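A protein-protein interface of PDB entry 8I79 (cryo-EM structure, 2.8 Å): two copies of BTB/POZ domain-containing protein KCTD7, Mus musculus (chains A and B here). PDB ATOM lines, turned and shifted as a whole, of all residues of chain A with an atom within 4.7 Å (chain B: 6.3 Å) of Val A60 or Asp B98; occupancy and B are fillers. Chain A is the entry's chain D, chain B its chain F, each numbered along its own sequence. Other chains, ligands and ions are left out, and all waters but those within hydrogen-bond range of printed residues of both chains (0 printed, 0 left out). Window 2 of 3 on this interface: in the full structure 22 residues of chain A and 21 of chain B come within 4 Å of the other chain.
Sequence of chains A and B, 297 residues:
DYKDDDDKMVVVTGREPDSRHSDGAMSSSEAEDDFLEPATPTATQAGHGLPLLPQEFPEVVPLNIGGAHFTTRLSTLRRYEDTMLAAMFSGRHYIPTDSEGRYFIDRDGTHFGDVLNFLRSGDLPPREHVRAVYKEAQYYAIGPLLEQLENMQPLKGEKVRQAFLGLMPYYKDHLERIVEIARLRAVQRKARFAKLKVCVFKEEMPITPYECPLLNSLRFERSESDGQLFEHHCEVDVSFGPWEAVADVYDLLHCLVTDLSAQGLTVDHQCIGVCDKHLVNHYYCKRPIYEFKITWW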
ATOM      1  N   PRO A  58       3.695   1.682 -25.458  1.00  0.00           N
ATOM      2  CA  PRO A  58       4.876   2.418 -25.003  1.00  0.00           C
ATOM      3  C   PRO A  58       5.726   2.853 -26.182  1.00  0.00           C
ATOM      4  O   PRO A  58       5.687   2.254 -27.259  1.00  0.00           O
ATOM      5  CB  PRO A  58       5.616   1.399 -24.128  1.00  0.00           C
ATOM      6  CG  PRO A  58       5.133   0.075 -24.603  1.00  0.00           C
ATOM      7  CD  PRO A  58       3.713   0.278 -25.018  1.00  0.00           C
ATOM      8  N   GLU A  59       6.495   3.923 -25.975  1.00  0.00           N
ATOM      9  CA  GLU A  59       7.391   4.386 -27.028  1.00  0.00           C
ATOM     10  C   GLU A  59       8.446   3.335 -27.345  1.00  0.00           C
ATOM     11  O   GLU A  59       8.830   3.160 -28.506  1.00  0.00           O
ATOM     12  CB  GLU A  59       8.042   5.708 -26.625  1.00  0.00           C
ATOM     13  CG  GLU A  59       7.062   6.865 -26.543  1.00  0.00           C
ATOM     14  CD  GLU A  59       6.426   7.188 -27.881  1.00  0.00           C
ATOM     15  OE1 GLU A  59       7.085   6.986 -28.922  1.00  0.00           O
ATOM     16  OE2 GLU A  59       5.261   7.638 -27.892  1.00  0.00           O
ATOM     17  N   VAL A  60       8.928   2.632 -26.326  1.00  0.00           N
ATOM     18  CA  VAL A  60       9.787   1.469 -26.510  1.00  0.00           C
ATOM     19  C   VAL A  60       8.899   0.235 -26.410  1.00  0.00           C
ATOM     20  O   VAL A  60       8.390  -0.086 -25.333  1.00  0.00           O
ATOM     21  CB  VAL A  60      10.912   1.433 -25.471  1.00  0.00           C
ATOM     22  CG1 VAL A  60      11.809   0.244 -25.713  1.00  0.00           C
ATOM     23  CG2 VAL A  60      11.710   2.719 -25.519  1.00  0.00           C
ATOM     24  N   VAL A  61       8.712  -0.457 -27.526  1.00  0.00           N
ATOM     25  CA  VAL A  61       7.773  -1.572 -27.619  1.00  0.00           C
ATOM     26  C   VAL A  61       8.541  -2.866 -27.383  1.00  0.00           C
ATOM     27  O   VAL A  61       9.399  -3.220 -28.203  1.00  0.00           O
ATOM     28  CB  VAL A  61       7.061  -1.598 -28.978  1.00  0.00           C
ATOM     29  CG1 VAL A  61       6.124  -2.782 -29.055  1.00  0.00           C
ATOM     30  CG2 VAL A  61       6.293  -0.318 -29.190  1.00  0.00           C
ATOM     31  N   PRO A  62       8.279  -3.589 -26.294  1.00  0.00           N
ATOM     32  CA  PRO A  62       8.889  -4.911 -26.108  1.00  0.00           C
ATOM     33  C   PRO A  62       8.170  -5.942 -26.966  1.00  0.00           C
ATOM     34  O   PRO A  62       6.940  -5.978 -27.009  1.00  0.00           O
ATOM     35  CB  PRO A  62       8.684  -5.184 -24.614  1.00  0.00           C
ATOM     36  CG  PRO A  62       8.332  -3.855 -24.016  1.00  0.00           C
ATOM     37  CD  PRO A  62       7.558  -3.167 -25.085  1.00  0.00           C
ATOM     38  N   THR A  71      13.288  -5.942 -29.041  1.00  0.00           N
ATOM     39  CA  THR A  71      12.832  -4.664 -28.518  1.00  0.00           C
ATOM     40  C   THR A  71      13.075  -3.593 -29.567  1.00  0.00           C
ATOM     41  O   THR A  71      14.150  -3.536 -30.169  1.00  0.00           O
ATOM     42  CB  THR A  71      13.550  -4.302 -27.213  1.00  0.00           C
ATOM     43  OG1 THR A  71      13.408  -5.374 -26.275  1.00  0.00           O
ATOM     44  CG2 THR A  71      12.958  -3.046 -26.612  1.00  0.00           C
ATOM     45  N   THR A  72      12.071  -2.750 -29.787  1.00  0.00           N
ATOM     46  CA  THR A  72      12.169  -1.702 -30.789  1.00  0.00           C
ATOM     47  C   THR A  72      11.223  -0.575 -30.411  1.00  0.00           C
ATOM     48  O   THR A  72      10.341  -0.737 -29.565  1.00  0.00           O
ATOM     49  CB  THR A  72      11.844  -2.231 -32.189  1.00  0.00           C
ATOM     50  OG1 THR A  72      12.202  -1.248 -33.167  1.00  0.00           O
ATOM     51  CG2 THR A  72      10.367  -2.535 -32.309  1.00  0.00           C
ATOM     52  N   ARG A  73      11.425   0.576 -31.038  1.00  0.00           N
ATOM     53  CA  ARG A  73      10.584   1.734 -30.785  1.00  0.00           C
ATOM     54  C   ARG A  73       9.283   1.629 -31.568  1.00  0.00           C
ATOM     55  O   ARG A  73       9.197   0.949 -32.591  1.00  0.00           O
ATOM     56  CB  ARG A  73      11.309   3.025 -31.156  1.00  0.00           C
ATOM     57  CG  ARG A  73      12.489   3.342 -30.267  1.00  0.00           C
ATOM     58  CD  ARG A  73      13.099   4.685 -30.602  1.00  0.00           C
ATOM     59  NE  ARG A  73      14.312   4.919 -29.832  1.00  0.00           N
ATOM     60  CZ  ARG A  73      14.331   5.412 -28.602  1.00  0.00           C
ATOM     61  NH1 ARG A  73      13.216   5.746 -27.974  1.00  0.00           N
ATOM     62  NH2 ARG A  73      15.499   5.570 -27.985  1.00  0.00           N
ATOM     63  N   LEU B  63      22.784  -2.345 -20.731  1.00  0.00           N
ATOM     64  CA  LEU B  63      22.477  -1.864 -22.069  1.00  0.00           C
ATOM     65  C   LEU B  63      21.583  -2.865 -22.779  1.00  0.00           C
ATOM     66  O   LEU B  63      21.780  -4.075 -22.655  1.00  0.00           O
ATOM     67  CB  LEU B  63      23.755  -1.639 -22.882  1.00  0.00           C
ATOM     68  CG  LEU B  63      24.520  -0.346 -22.615  1.00  0.00           C
ATOM     69  CD1 LEU B  63      25.792  -0.326 -23.432  1.00  0.00           C
ATOM     70  CD2 LEU B  63      23.657   0.856 -22.933  1.00  0.00           C
ATOM     71  N   ASN B  64      20.604  -2.353 -23.514  1.00  0.00           N
ATOM     72  CA  ASN B  64      19.720  -3.161 -24.344  1.00  0.00           C
ATOM     73  C   ASN B  64      19.809  -2.620 -25.764  1.00  0.00           C
ATOM     74  O   ASN B  64      19.209  -1.590 -26.080  1.00  0.00           O
ATOM     75  CB  ASN B  64      18.288  -3.114 -23.821  1.00  0.00           C
ATOM     76  CG  ASN B  64      17.360  -4.024 -24.587  1.00  0.00           C
ATOM     77  OD1 ASN B  64      17.794  -4.996 -25.200  1.00  0.00           O
ATOM     78  ND2 ASN B  64      16.074  -3.715 -24.558  1.00  0.00           N
ATOM     79  N   HIS B  69      21.245  -7.964 -24.817  1.00  0.00           N
ATOM     80  CA  HIS B  69      21.605  -7.465 -23.496  1.00  0.00           C
ATOM     81  C   HIS B  69      23.119  -7.384 -23.367  1.00  0.00           C
ATOM     82  O   HIS B  69      23.812  -8.402 -23.466  1.00  0.00           O
ATOM     83  CB  HIS B  69      21.022  -8.358 -22.404  1.00  0.00           C
ATOM     84  CG  HIS B  69      19.551  -8.183 -22.205  1.00  0.00           C
ATOM     85  ND1 HIS B  69      18.849  -8.842 -21.219  1.00  0.00           N
ATOM     86  CD2 HIS B  69      18.647  -7.422 -22.864  1.00  0.00           C
ATOM     87  CE1 HIS B  69      17.577  -8.494 -21.280  1.00  0.00           C
ATOM     88  NE2 HIS B  69      17.428  -7.633 -22.269  1.00  0.00           N
ATOM     89  N   PRO B  96      15.754   6.568 -22.338  1.00  0.00           N
ATOM     90  CA  PRO B  96      14.598   5.781 -21.891  1.00  0.00           C
ATOM     91  C   PRO B  96      14.997   4.363 -21.513  1.00  0.00           C
ATOM     92  O   PRO B  96      15.762   3.705 -22.220  1.00  0.00           O
ATOM     93  CB  PRO B  96      13.671   5.796 -23.113  1.00  0.00           C
ATOM     94  CG  PRO B  96      14.565   6.127 -24.297  1.00  0.00           C
ATOM     95  CD  PRO B  96      15.943   6.471 -23.793  1.00  0.00           C
ATOM     96  N   THR B  97      14.462   3.895 -20.392  1.00  0.00           N
ATOM     97  CA  THR B  97      14.595   2.509 -19.973  1.00  0.00           C
ATOM     98  C   THR B  97      13.443   1.687 -20.544  1.00  0.00           C
ATOM     99  O   THR B  97      12.423   2.221 -20.985  1.00  0.00           O
ATOM    100  CB  THR B  97      14.630   2.408 -18.447  1.00  0.00           C
ATOM    101  OG1 THR B  97      13.642   3.281 -17.887  1.00  0.00           O
ATOM    102  CG2 THR B  97      15.997   2.812 -17.926  1.00  0.00           C
ATOM    103  N   ASP B  98      13.614   0.365 -20.531  1.00  0.00           N
ATOM    104  CA  ASP B  98      12.684  -0.550 -21.193  1.00  0.00           C
ATOM    105  C   ASP B  98      12.235  -1.643 -20.218  1.00  0.00           C
ATOM    106  O   ASP B  98      12.815  -2.729 -20.154  1.00  0.00           O
ATOM    107  CB  ASP B  98      13.320  -1.139 -22.450  1.00  0.00           C
ATOM    108  CG  ASP B  98      14.707  -1.695 -22.198  1.00  0.00           C
ATOM    109  OD1 ASP B  98      15.378  -2.070 -23.178  1.00  0.00           O
ATOM    110  OD2 ASP B  98      15.136  -1.740 -21.028  1.00  0.00           O
ATOM    111  N   SER B  99      11.183  -1.350 -19.452  1.00  0.00           N
ATOM    112  CA  SER B  99      10.510  -2.278 -18.546  1.00  0.00           C
ATOM    113  C   SER B  99      11.429  -2.801 -17.452  1.00  0.00           C
ATOM    114  O   SER B  99      10.994  -3.618 -16.632  1.00  0.00           O
ATOM    115  CB  SER B  99       9.886  -3.471 -19.286  1.00  0.00           C
ATOM    116  OG  SER B  99      10.884  -4.324 -19.818  1.00  0.00           O
ATOM    117  N   GLU B 100      12.682  -2.359 -17.411  1.00  0.00           N
ATOM    118  CA  GLU B 100      13.665  -2.818 -16.443  1.00  0.00           C
ATOM    119  C   GLU B 100      14.833  -1.847 -16.485  1.00  0.00           C
ATOM    120  O   GLU B 100      14.853  -0.911 -17.286  1.00  0.00           O
ATOM    121  CB  GLU B 100      14.112  -4.253 -16.737  1.00  0.00           C
ATOM    122  CG  GLU B 100      14.793  -4.425 -18.079  1.00  0.00           C
ATOM    123  CD  GLU B 100      15.070  -5.877 -18.405  1.00  0.00           C
ATOM    124  OE1 GLU B 100      14.718  -6.749 -17.583  1.00  0.00           O
ATOM    125  OE2 GLU B 100      15.630  -6.149 -19.488  1.00  0.00           O
ATOM    126  N   GLY B 101      15.809  -2.080 -15.616  1.00  0.00           N
ATOM    127  CA  GLY B 101      16.907  -1.142 -15.497  1.00  0.00           C
ATOM    128  C   GLY B 101      17.917  -1.212 -16.623  1.00  0.00           C
ATOM    129  O   GLY B 101      19.125  -1.193 -16.373  1.00  0.00           O
ATOM    130  N   ARG B 102      17.445  -1.274 -17.864  1.00  0.00           N
ATOM    131  CA  ARG B 102      18.307  -1.311 -19.035  1.00  0.00           C
ATOM    132  C   ARG B 102      18.026  -0.110 -19.923  1.00  0.00           C
ATOM    133  O   ARG B 102      16.886   0.346 -20.034  1.00  0.00           O
ATOM    134  CB  ARG B 102      18.108  -2.601 -19.835  1.00  0.00           C
ATOM    135  CG  ARG B 102      18.367  -3.871 -19.051  1.00  0.00           C
ATOM    136  CD  ARG B 102      18.637  -5.038 -19.982  1.00  0.00           C
ATOM    137  NE  ARG B 102      20.050  -5.393 -20.033  1.00  0.00           N
ATOM    138  CZ  ARG B 102      20.708  -5.997 -19.055  1.00  0.00           C
ATOM    139  NH1 ARG B 102      20.108  -6.345 -17.929  1.00  0.00           N
ATOM    140  NH2 ARG B 102      22.001  -6.265 -19.211  1.00  0.00           N
ATOM    141  N   TYR B 103      19.075   0.401 -20.557  1.00  0.00           N
ATOM    142  CA  TYR B 103      18.968   1.553 -21.437  1.00  0.00           C
ATOM    143  C   TYR B 103      18.906   1.088 -22.884  1.00  0.00           C
ATOM    144  O   TYR B 103      19.722   0.274 -23.322  1.00  0.00           O
ATOM    145  CB  TYR B 103      20.143   2.507 -21.229  1.00  0.00           C
ATOM    146  CG  TYR B 103      20.197   3.073 -19.832  1.00  0.00           C
ATOM    147  CD1 TYR B 103      20.933   2.448 -18.837  1.00  0.00           C
ATOM    148  CD2 TYR B 103      19.493   4.218 -19.500  1.00  0.00           C
ATOM    149  CE1 TYR B 103      20.978   2.956 -17.559  1.00  0.00           C
ATOM    150  CE2 TYR B 103      19.530   4.732 -18.225  1.00  0.00           C
ATOM    151  CZ  TYR B 103      20.273   4.097 -17.259  1.00  0.00           C
ATOM    152  OH  TYR B 103      20.309   4.612 -15.985  1.00  0.00           O
ATOM    153  N   PHE B 104      17.936   1.615 -23.623  1.00  0.00           N
ATOM    154  CA  PHE B 104      17.577   1.093 -24.933  1.00  0.00           C
ATOM    155  C   PHE B 104      18.247   1.888 -26.046  1.00  0.00           C
ATOM    156  O   PHE B 104      18.207   3.122 -26.048  1.00  0.00           O
ATOM    157  CB  PHE B 104      16.061   1.115 -25.118  1.00  0.00           C
ATOM    158  CG  PHE B 104      15.615   0.612 -26.452  1.00  0.00           C
ATOM    159  CD1 PHE B 104      15.964  -0.652 -26.878  1.00  0.00           C
ATOM    160  CD2 PHE B 104      14.859   1.411 -27.286  1.00  0.00           C
ATOM    161  CE1 PHE B 104      15.563  -1.111 -28.106  1.00  0.00           C
ATOM    162  CE2 PHE B 104      14.457   0.957 -28.513  1.00  0.00           C
ATOM    163  CZ  PHE B 104      14.809  -0.305 -28.925  1.00  0.00           C
ATOM    164  N   ILE B 105      18.862   1.171 -26.986  1.00  0.00           N
ATOM    165  CA  ILE B 105      19.344   1.733 -28.243  1.00  0.00           C
ATOM    166  C   ILE B 105      18.736   0.921 -29.376  1.00  0.00           C
ATOM    167  O   ILE B 105      18.976  -0.287 -29.477  1.00  0.00           O
ATOM    168  CB  ILE B 105      20.880   1.720 -28.331  1.00  0.00           C
ATOM    169  CG1 ILE B 105      21.495   2.431 -27.128  1.00  0.00           C
ATOM    170  CG2 ILE B 105      21.338   2.364 -29.624  1.00  0.00           C
ATOM    171  CD1 ILE B 105      22.987   2.624 -27.236  1.00  0.00           C
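Among the printed residues, merely in contact across the chains: Val A60 with Asp B98 (3.9 Å), Val A60 with Phe B104 (3.6 Å), Thr A71 with Asn B64 (3.6 Å), Thr A71 with Phe B104 (3.5 Å), Thr A72 with Phe B104 (3.5 Å), Arg A73 with Pro B96 (3.8 Å) and Arg A73 with Phe B104 (3.6 Å).
Of the 8 printed residues of chain A, 4 touch a printed residue of chain B.
Along chain A the printed residues that touch a printed residue of chain B span positions 60 to 73.
Printed residues of chain B that touch a printed residue of chain A: Asn B64, Pro B96, Asp B98 and Phe B104.
Hydrophobic or aromatic side chains of chain B that line the printed part of chain A: Pro B96 and Phe B104.
Among the printed residues, 7 pairs touch across the chains.
Asp B98 touches just one residue of chain A: Val A60.
Printed residues of chain B within 4 Å of Thr A72: Phe B104 (3.5 Å).
Of the printed residues of chain B, Arg A73 touches Pro B96 (3.8 Å) and Phe B104 (3.6 Å).
Printed residues of chain A within 4 Å of Asn B64: Thr A71 (3.6 Å).
Of the printed residues of chain B, Thr A71 touches Asn B64 (3.6 Å) and Phe B104 (3.5 Å).
Of the printed residues of chain A, Phe B104 touches Val A60, Thr A71, Thr A72 and Arg A73.
Leu B63 touches none of the printed residues of chain A.
The nearest residue of chain B that does not touch Val A60 is Pro B96 (4.4 Å).
No position is printed for both chains.
N of Asn B64 is in hydrogen-bond range of O of Tyr B103.
The backbone carbonyl oxygen (O) of Pro B96 sits at hydrogen-bond distance from the backbone NH (N) of Phe B104, 3.3 Å away.
O of Asn B64 sits at hydrogen-bond distance from N of Ile B105.
The backbone NH of Val A61 lies within hydrogen-bond range of the backbone carbonyl oxygen of Thr A72, 2.6 Å away.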
